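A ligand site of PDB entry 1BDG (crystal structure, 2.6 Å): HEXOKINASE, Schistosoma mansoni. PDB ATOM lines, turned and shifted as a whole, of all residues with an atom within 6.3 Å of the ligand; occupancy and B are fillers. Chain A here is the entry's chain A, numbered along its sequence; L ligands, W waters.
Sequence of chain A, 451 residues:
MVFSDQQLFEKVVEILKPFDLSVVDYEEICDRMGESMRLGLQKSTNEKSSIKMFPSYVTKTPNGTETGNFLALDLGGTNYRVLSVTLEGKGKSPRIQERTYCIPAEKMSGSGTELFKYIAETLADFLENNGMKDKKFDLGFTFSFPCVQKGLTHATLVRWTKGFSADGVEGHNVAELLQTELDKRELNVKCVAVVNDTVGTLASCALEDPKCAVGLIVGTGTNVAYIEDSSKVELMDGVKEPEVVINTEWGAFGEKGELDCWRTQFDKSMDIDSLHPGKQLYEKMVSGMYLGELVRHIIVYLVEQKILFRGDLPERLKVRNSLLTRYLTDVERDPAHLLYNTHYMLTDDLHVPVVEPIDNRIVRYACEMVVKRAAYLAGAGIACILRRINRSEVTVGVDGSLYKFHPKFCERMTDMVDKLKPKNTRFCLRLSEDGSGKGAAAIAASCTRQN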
ATOM      1  N   GLY A  76      20.916 -13.014 -27.931  1.00  0.00           N
ATOM      2  CA  GLY A  76      19.513 -12.646 -28.029  1.00  0.00           C
ATOM      3  C   GLY A  76      19.181 -11.896 -29.296  1.00  0.00           C
ATOM      4  O   GLY A  76      18.112 -12.115 -29.883  1.00  0.00           O
ATOM      5  N   GLY A  77      20.101 -11.019 -29.720  1.00  0.00           N
ATOM      6  CA  GLY A  77      19.918 -10.197 -30.916  1.00  0.00           C
ATOM      7  C   GLY A  77      19.940 -10.978 -32.212  1.00  0.00           C
ATOM      8  O   GLY A  77      19.818 -12.204 -32.189  1.00  0.00           O
ATOM      9  N   PHE A 143      22.957 -10.146 -22.144  1.00  0.00           N
ATOM     10  CA  PHE A 143      21.899 -11.159 -22.265  1.00  0.00           C
ATOM     11  C   PHE A 143      20.603 -10.416 -22.575  1.00  0.00           C
ATOM     12  O   PHE A 143      19.961  -9.882 -21.673  1.00  0.00           O
ATOM     13  CB  PHE A 143      21.789 -11.924 -20.946  1.00  0.00           C
ATOM     14  CG  PHE A 143      20.951 -13.172 -21.039  1.00  0.00           C
ATOM     15  CD1 PHE A 143      21.170 -14.100 -22.054  1.00  0.00           C
ATOM     16  CD2 PHE A 143      19.975 -13.439 -20.076  1.00  0.00           C
ATOM     17  CE1 PHE A 143      20.433 -15.290 -22.108  1.00  0.00           C
ATOM     18  CE2 PHE A 143      19.246 -14.619 -20.112  1.00  0.00           C
ATOM     19  CZ  PHE A 143      19.475 -15.553 -21.134  1.00  0.00           C
ATOM     20  N   SER A 144      20.233 -10.392 -23.849  1.00  0.00           N
ATOM     21  CA  SER A 144      19.041  -9.691 -24.304  1.00  0.00           C
ATOM     22  C   SER A 144      17.714 -10.235 -23.805  1.00  0.00           C
ATOM     23  O   SER A 144      16.802 -10.463 -24.606  1.00  0.00           O
ATOM     24  CB  SER A 144      18.992  -9.706 -25.832  1.00  0.00           C
ATOM     25  OG  SER A 144      20.253  -9.429 -26.384  1.00  0.00           O
ATOM     26  N   PHE A 145      17.542 -10.416 -22.498  1.00  0.00           N
ATOM     27  CA  PHE A 145      16.269 -10.926 -22.007  1.00  0.00           C
ATOM     28  C   PHE A 145      15.913 -10.324 -20.660  1.00  0.00           C
ATOM     29  O   PHE A 145      16.786  -9.772 -19.984  1.00  0.00           O
ATOM     30  CB  PHE A 145      16.296 -12.473 -21.938  1.00  0.00           C
ATOM     31  CG  PHE A 145      16.394 -13.140 -23.282  1.00  0.00           C
ATOM     32  CD1 PHE A 145      15.280 -13.260 -24.096  1.00  0.00           C
ATOM     33  CD2 PHE A 145      17.617 -13.597 -23.763  1.00  0.00           C
ATOM     34  CE1 PHE A 145      15.387 -13.814 -25.358  1.00  0.00           C
ATOM     35  CE2 PHE A 145      17.724 -14.152 -25.025  1.00  0.00           C
ATOM     36  CZ  PHE A 145      16.609 -14.254 -25.815  1.00  0.00           C
ATOM     37  N   PRO A 146      14.627 -10.387 -20.266  1.00  0.00           N
ATOM     38  CA  PRO A 146      14.215  -9.827 -18.979  1.00  0.00           C
ATOM     39  C   PRO A 146      14.790 -10.675 -17.873  1.00  0.00           C
ATOM     40  O   PRO A 146      14.608 -11.890 -17.849  1.00  0.00           O
ATOM     41  CB  PRO A 146      12.693  -9.982 -19.035  1.00  0.00           C
ATOM     42  CG  PRO A 146      12.515 -11.216 -19.821  1.00  0.00           C
ATOM     43  CD  PRO A 146      13.496 -11.023 -20.950  1.00  0.00           C
ATOM     44  N   ARG A 159      11.840 -14.753 -18.198  1.00  0.00           N
ATOM     45  CA  ARG A 159      11.215 -15.541 -19.242  1.00  0.00           C
ATOM     46  C   ARG A 159      11.944 -15.381 -20.572  1.00  0.00           C
ATOM     47  O   ARG A 159      12.699 -14.434 -20.751  1.00  0.00           O
ATOM     48  CB  ARG A 159       9.736 -15.162 -19.377  1.00  0.00           C
ATOM     49  CG  ARG A 159       9.494 -13.734 -19.839  1.00  0.00           C
ATOM     50  CD  ARG A 159       8.016 -13.391 -19.757  1.00  0.00           C
ATOM     51  NE  ARG A 159       7.730 -12.190 -20.515  1.00  0.00           N
ATOM     52  CZ  ARG A 159       6.542 -11.603 -20.579  1.00  0.00           C
ATOM     53  NH1 ARG A 159       5.494 -12.107 -19.932  1.00  0.00           N
ATOM     54  NH2 ARG A 159       6.394 -10.513 -21.289  1.00  0.00           N
ATOM     55  N   TRP A 160      11.778 -16.364 -21.453  1.00  0.00           N
ATOM     56  CA  TRP A 160      12.422 -16.322 -22.745  1.00  0.00           C
ATOM     57  C   TRP A 160      11.483 -15.577 -23.673  1.00  0.00           C
ATOM     58  O   TRP A 160      10.270 -15.845 -23.680  1.00  0.00           O
ATOM     59  CB  TRP A 160      12.612 -17.731 -23.339  1.00  0.00           C
ATOM     60  CG  TRP A 160      13.818 -18.536 -22.909  1.00  0.00           C
ATOM     61  CD1 TRP A 160      13.791 -19.768 -22.344  1.00  0.00           C
ATOM     62  CD2 TRP A 160      15.211 -18.223 -23.102  1.00  0.00           C
ATOM     63  NE1 TRP A 160      15.068 -20.247 -22.190  1.00  0.00           N
ATOM     64  CE2 TRP A 160      15.957 -19.317 -22.652  1.00  0.00           C
ATOM     65  CE3 TRP A 160      15.890 -17.122 -23.633  1.00  0.00           C
ATOM     66  CZ2 TRP A 160      17.364 -19.358 -22.701  1.00  0.00           C
ATOM     67  CZ3 TRP A 160      17.298 -17.156 -23.687  1.00  0.00           C
ATOM     68  CH2 TRP A 160      18.010 -18.266 -23.216  1.00  0.00           C
ATOM     69  N   THR A 161      12.035 -14.626 -24.424  1.00  0.00           N
ATOM     70  CA  THR A 161      11.251 -13.890 -25.385  1.00  0.00           C
ATOM     71  C   THR A 161      11.888 -14.237 -26.716  1.00  0.00           C
ATOM     72  O   THR A 161      12.871 -14.996 -26.743  1.00  0.00           O
ATOM     73  CB  THR A 161      11.335 -12.376 -25.146  1.00  0.00           C
ATOM     74  OG1 THR A 161      12.685 -11.928 -25.312  1.00  0.00           O
ATOM     75  CG2 THR A 161      10.860 -12.031 -23.742  1.00  0.00           C
ATOM     76  N   LYS A 162      11.311 -13.768 -27.809  1.00  0.00           N
ATOM     77  CA  LYS A 162      11.864 -14.025 -29.134  1.00  0.00           C
ATOM     78  C   LYS A 162      11.814 -15.478 -29.618  1.00  0.00           C
ATOM     79  O   LYS A 162      10.792 -16.144 -29.464  1.00  0.00           O
ATOM     80  CB  LYS A 162      13.277 -13.430 -29.226  1.00  0.00           C
ATOM     81  CG  LYS A 162      13.268 -11.906 -29.290  1.00  0.00           C
ATOM     82  CD  LYS A 162      14.626 -11.307 -29.425  1.00  0.00           C
ATOM     83  CE  LYS A 162      15.305 -11.192 -28.104  1.00  0.00           C
ATOM     84  NZ  LYS A 162      16.386 -10.158 -28.164  1.00  0.00           N
ATOM     85  N   ASN A 196      21.717  -6.071 -20.000  1.00  0.00           N
ATOM     86  CA  ASN A 196      20.732  -6.225 -21.072  1.00  0.00           C
ATOM     87  C   ASN A 196      21.268  -5.451 -22.310  1.00  0.00           C
ATOM     88  O   ASN A 196      22.094  -4.542 -22.182  1.00  0.00           O
ATOM     89  CB  ASN A 196      19.394  -5.670 -20.581  1.00  0.00           C
ATOM     90  CG  ASN A 196      18.271  -5.894 -21.555  1.00  0.00           C
ATOM     91  OD1 ASN A 196      17.898  -5.000 -22.305  1.00  0.00           O
ATOM     92  ND2 ASN A 196      17.727  -7.094 -21.541  1.00  0.00           N
ATOM     93  N   ASP A 197      20.810  -5.776 -23.511  1.00  0.00           N
ATOM     94  CA  ASP A 197      21.322  -5.039 -24.665  1.00  0.00           C
ATOM     95  C   ASP A 197      21.013  -3.550 -24.616  1.00  0.00           C
ATOM     96  O   ASP A 197      21.892  -2.747 -24.907  1.00  0.00           O
ATOM     97  CB  ASP A 197      20.887  -5.663 -26.000  1.00  0.00           C
ATOM     98  CG  ASP A 197      19.390  -5.870 -26.127  1.00  0.00           C
ATOM     99  OD1 ASP A 197      18.599  -5.223 -25.420  1.00  0.00           O
ATOM    100  OD2 ASP A 197      18.969  -6.683 -26.959  1.00  0.00           O
ATOM    101  N   THR A 198      19.821  -3.157 -24.186  1.00  0.00           N
ATOM    102  CA  THR A 198      19.484  -1.735 -24.118  1.00  0.00           C
ATOM    103  C   THR A 198      20.475  -1.005 -23.217  1.00  0.00           C
ATOM    104  O   THR A 198      21.001   0.052 -23.595  1.00  0.00           O
ATOM    105  CB  THR A 198      18.118  -1.534 -23.545  1.00  0.00           C
ATOM    106  OG1 THR A 198      17.992  -2.352 -22.384  1.00  0.00           O
ATOM    107  CG2 THR A 198      17.066  -1.928 -24.557  1.00  0.00           C
ATOM    108  N   ILE A 217      16.472  -0.161 -28.583  1.00  0.00           N
ATOM    109  CA  ILE A 217      16.734  -1.324 -29.448  1.00  0.00           C
ATOM    110  C   ILE A 217      15.510  -1.629 -30.313  1.00  0.00           C
ATOM    111  O   ILE A 217      14.451  -1.962 -29.795  1.00  0.00           O
ATOM    112  CB  ILE A 217      17.081  -2.600 -28.659  1.00  0.00           C
ATOM    113  CG1 ILE A 217      18.456  -2.479 -27.998  1.00  0.00           C
ATOM    114  CG2 ILE A 217      17.064  -3.788 -29.574  1.00  0.00           C
ATOM    115  CD1 ILE A 217      19.604  -2.370 -28.976  1.00  0.00           C
ATOM    116  N   VAL A 218      15.631  -1.447 -31.613  1.00  0.00           N
ATOM    117  CA  VAL A 218      14.555  -1.751 -32.530  1.00  0.00           C
ATOM    118  C   VAL A 218      15.113  -2.701 -33.604  1.00  0.00           C
ATOM    119  O   VAL A 218      15.441  -2.308 -34.719  1.00  0.00           O
ATOM    120  CB  VAL A 218      13.896  -0.449 -33.139  1.00  0.00           C
ATOM    121  CG1 VAL A 218      13.065   0.261 -32.054  1.00  0.00           C
ATOM    122  CG2 VAL A 218      14.937   0.527 -33.659  1.00  0.00           C
ATOM    123  N   GLY A 219      15.276  -3.959 -33.214  1.00  0.00           N
ATOM    124  CA  GLY A 219      15.829  -4.965 -34.118  1.00  0.00           C
ATOM    125  C   GLY A 219      14.988  -6.213 -34.103  1.00  0.00           C
ATOM    126  O   GLY A 219      13.791  -6.132 -34.345  1.00  0.00           O
ATOM    127  N   THR A 220      15.590  -7.369 -33.837  1.00  0.00           N
ATOM    128  CA  THR A 220      14.825  -8.621 -33.791  1.00  0.00           C
ATOM    129  C   THR A 220      13.688  -8.428 -32.775  1.00  0.00           C
ATOM    130  O   THR A 220      12.575  -8.944 -32.946  1.00  0.00           O
ATOM    131  CB  THR A 220      15.720  -9.835 -33.395  1.00  0.00           C
ATOM    132  OG1 THR A 220      16.704 -10.061 -34.423  1.00  0.00           O
ATOM    133  CG2 THR A 220      14.901 -11.110 -33.251  1.00  0.00           C
ATOM    134  N   GLY A 221      13.963  -7.564 -31.793  1.00  0.00           N
ATOM    135  CA  GLY A 221      13.026  -7.229 -30.752  1.00  0.00           C
ATOM    136  C   GLY A 221      13.137  -5.764 -30.345  1.00  0.00           C
ATOM    137  O   GLY A 221      14.125  -5.123 -30.653  1.00  0.00           O
ATOM    138  N   THR A 222      12.120  -5.232 -29.683  1.00  0.00           N
ATOM    139  CA  THR A 222      12.152  -3.844 -29.266  1.00  0.00           C
ATOM    140  C   THR A 222      12.160  -3.736 -27.754  1.00  0.00           C
ATOM    141  O   THR A 222      11.552  -4.573 -27.047  1.00  0.00           O
ATOM    142  CB  THR A 222      11.001  -3.017 -29.888  1.00  0.00           C
ATOM    143  OG1 THR A 222      11.176  -1.633 -29.568  1.00  0.00           O
ATOM    144  CG2 THR A 222       9.640  -3.462 -29.374  1.00  0.00           C
ATOM    145  N   ASN A 223      12.897  -2.759 -27.254  1.00  0.00           N
ATOM    146  CA  ASN A 223      13.019  -2.496 -25.828  1.00  0.00           C
ATOM    147  C   ASN A 223      13.847  -1.231 -25.638  1.00  0.00           C
ATOM    148  O   ASN A 223      14.645  -0.888 -26.495  1.00  0.00           O
ATOM    149  CB  ASN A 223      13.697  -3.674 -25.121  1.00  0.00           C
ATOM    150  CG  ASN A 223      13.627  -3.565 -23.627  1.00  0.00           C
ATOM    151  OD1 ASN A 223      13.021  -2.655 -23.098  1.00  0.00           O
ATOM    152  ND2 ASN A 223      14.257  -4.497 -22.943  1.00  0.00           N
ATOM    153  N   VAL A 224      13.630  -0.523 -24.536  1.00  0.00           N
ATOM    154  CA  VAL A 224      14.351   0.698 -24.238  1.00  0.00           C
ATOM    155  C   VAL A 224      14.817   0.633 -22.785  1.00  0.00           C
ATOM    156  O   VAL A 224      14.244  -0.099 -21.965  1.00  0.00           O
ATOM    157  CB  VAL A 224      13.459   1.943 -24.388  1.00  0.00           C
ATOM    158  CG1 VAL A 224      12.652   2.192 -23.135  1.00  0.00           C
ATOM    159  CG2 VAL A 224      14.291   3.142 -24.697  1.00  0.00           C
ATOM    160  N   ASN A 247      15.635  -1.123 -17.011  1.00  0.00           N
ATOM    161  CA  ASN A 247      15.369  -1.931 -18.199  1.00  0.00           C
ATOM    162  C   ASN A 247      13.845  -2.058 -18.213  1.00  0.00           C
ATOM    163  O   ASN A 247      13.236  -2.850 -17.475  1.00  0.00           O
ATOM    164  CB  ASN A 247      16.030  -3.295 -18.067  1.00  0.00           C
ATOM    165  CG  ASN A 247      15.678  -4.230 -19.211  1.00  0.00           C
ATOM    166  OD1 ASN A 247      15.148  -3.821 -20.236  1.00  0.00           O
ATOM    167  ND2 ASN A 247      15.988  -5.497 -19.035  1.00  0.00           N
ATOM    168  N   GLU A 249      11.680  -3.080 -20.565  1.00  0.00           N
ATOM    169  CA  GLU A 249      11.201  -4.361 -21.060  1.00  0.00           C
ATOM    170  C   GLU A 249       9.736  -4.133 -21.491  1.00  0.00           C
ATOM    171  O   GLU A 249       8.819  -4.850 -21.079  1.00  0.00           O
ATOM    172  CB  GLU A 249      11.346  -5.422 -19.958  1.00  0.00           C
ATOM    173  CG  GLU A 249      11.419  -6.860 -20.444  1.00  0.00           C
ATOM    174  CD  GLU A 249      12.580  -7.155 -21.389  1.00  0.00           C
ATOM    175  OE1 GLU A 249      13.758  -7.090 -20.969  1.00  0.00           O
ATOM    176  OE2 GLU A 249      12.310  -7.490 -22.559  1.00  0.00           O
ATOM    177  N   GLY A 251       8.435  -4.565 -24.404  1.00  0.00           N
ATOM    178  CA  GLY A 251       7.884  -5.470 -25.388  1.00  0.00           C
ATOM    179  C   GLY A 251       6.639  -6.096 -24.792  1.00  0.00           C
ATOM    180  O   GLY A 251       5.696  -6.436 -25.494  1.00  0.00           O
ATOM    181  N   GLN A 280       4.575 -10.453 -25.028  1.00  0.00           N
ATOM    182  CA  GLN A 280       5.268  -9.420 -25.802  1.00  0.00           C
ATOM    183  C   GLN A 280       4.396  -8.815 -26.872  1.00  0.00           C
ATOM    184  O   GLN A 280       4.845  -8.552 -27.988  1.00  0.00           O
ATOM    185  CB  GLN A 280       6.563  -9.960 -26.427  1.00  0.00           C
ATOM    186  CG  GLN A 280       7.500 -10.684 -25.466  1.00  0.00           C
ATOM    187  CD  GLN A 280       8.267  -9.777 -24.517  1.00  0.00           C
ATOM    188  OE1 GLN A 280       8.200  -9.929 -23.306  1.00  0.00           O
ATOM    189  NE2 GLN A 280       9.046  -8.870 -25.079  1.00  0.00           N
ATOM    190  N   GLU A 283       5.721  -5.672 -28.620  1.00  0.00           N
ATOM    191  CA  GLU A 283       6.866  -5.997 -29.450  1.00  0.00           C
ATOM    192  C   GLU A 283       6.476  -6.578 -30.800  1.00  0.00           C
ATOM    193  O   GLU A 283       7.087  -6.286 -31.815  1.00  0.00           O
ATOM    194  CB  GLU A 283       7.804  -6.965 -28.746  1.00  0.00           C
ATOM    195  CG  GLU A 283       8.856  -7.549 -29.660  1.00  0.00           C
ATOM    196  CD  GLU A 283       9.864  -8.362 -28.924  1.00  0.00           C
ATOM    197  OE1 GLU A 283       9.572  -9.543 -28.640  1.00  0.00           O
ATOM    198  OE2 GLU A 283      10.944  -7.824 -28.636  1.00  0.00           O
HETATM  199  C1  LIG L   1      13.325  -8.658 -26.489  1.00  0.00           C
HETATM  200  C2  LIG L   1      13.902  -8.994 -25.124  1.00  0.00           C
HETATM  201  C3  LIG L   1      14.504  -7.745 -24.503  1.00  0.00           C
HETATM  202  C4  LIG L   1      15.526  -7.150 -25.455  1.00  0.00           C
HETATM  203  C5  LIG L   1      14.871  -6.860 -26.782  1.00  0.00           C
HETATM  204  C6  LIG L   1      15.857  -6.315 -27.799  1.00  0.00           C
HETATM  205  O1  LIG L   1      12.366  -7.668 -26.327  1.00  0.00           O
HETATM  206  O2  LIG L   1      12.887  -9.501 -24.256  1.00  0.00           O
HETATM  207  O3  LIG L   1      15.127  -8.065 -23.267  1.00  0.00           O
HETATM  208  O4  LIG L   1      16.061  -5.970 -24.900  1.00  0.00           O
HETATM  209  O5  LIG L   1      14.333  -8.065 -27.320  1.00  0.00           O
HETATM  210  O6  LIG L   1      16.530  -7.353 -28.467  1.00  0.00           O
HETATM  211  O   HOH W   1      10.561  -6.012 -24.241  1.00  0.00           O
HETATM  212  O   HOH W   2      16.737  -7.685 -31.083  1.00  0.00           O
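Water W2 lies within hydrogen-bond range of an oxygen (O6) of the ligand (2.6 Å), the backbone NH (N) of Gly 221 (2.9 Å) and the backbone NH (N) of Thr 220 (3.0 Å).
Water W1 lies within hydrogen-bond range of N of Gly 251 (2.6 Å), OE2 of Glu 249 (2.8 Å), O1 of the ligand (3.2 Å), O of Thr 222 (3.3 Å) and NE2 of Gln 280 (3.3 Å).
ND2 of Asn 223 lies within hydrogen-bond range of O4 of the ligand, at 3.0 Å.
The side-chain carboxylate (OE2) of Glu 283 lies within hydrogen-bond range of an oxygen (O1) of the ligand (2.7 Å).
An oxygen (O3) of the ligand sits at hydrogen-bond distance from the backbone carbonyl oxygen (O) of Ser 144.
The side-chain amide nitrogen of Asn 196 sits at hydrogen-bond distance from an oxygen (O3) of the ligand (3.3 Å).
OD1 of Asp 197 sits at hydrogen-bond distance from O4 of the ligand (2.7 Å).
An oxygen (O1) of the ligand lies within hydrogen-bond range of the backbone carbonyl oxygen (O) of Thr 222 (3.3 Å).
The side-chain amino group of Lys 162 lies within hydrogen-bond range of an oxygen (O6) of the ligand (2.8 Å).
An oxygen (O2) of the ligand lies within hydrogen-bond range of the side-chain carboxylate (OE2) of Glu 249.
O2 of the ligand is in hydrogen-bond range of OG1 of Thr 161.
The backbone NH (N) of Phe 145 sits close to an oxygen (O3) of the ligand (3.5 Å).
The side-chain amide nitrogen (ND2) of Asn 196 sits close to the side-chain amide nitrogen (ND2) of Asn 247 (3.4 Å).
The side-chain hydroxyl (OG) of Ser 144 is in hydrogen-bond range of the side-chain carboxylate (OD2) of Asp 197 (3.1 Å).
The side-chain carboxylate of Glu 249 lies within hydrogen-bond range of the side-chain amide nitrogen of Asn 247.
The backbone NH (N) of Ile 217 sits at hydrogen-bond distance from the backbone carbonyl oxygen (O) of Asn 223 (2.9 Å).
The side-chain amino group (NZ) of Lys 162 sits at hydrogen-bond distance from the backbone carbonyl oxygen (O) of Gly 76 (3.1 Å).
The backbone NH (N) of Glu 283 lies within hydrogen-bond range of the backbone carbonyl oxygen (O) of Gly 251 (3.2 Å).
OE1 of Gln 280 sits at hydrogen-bond distance from NH2 of Arg 159 (2.8 Å).
OD1 of Asn 196 lies within hydrogen-bond range of OG1 of Thr 198 (2.7 Å).
Residues that only touch the ligand: Pro 146 (3.7 Å), Ile 217 (3.3 Å), Gly 221 (3.5 Å) and Gln 280 (3.7 Å).
Hydrophobic or aromatic side chains that line the ligand: Pro 146 and Ile 217.
Within 4 Å of the ligand: Ser 144, Phe 145, Pro 146, Thr 161, Lys 162, Asn 196, Asp 197, Ile 217, Gly 221, Thr 222, Asn 223, Glu 249, Gln 280 and Glu 283.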
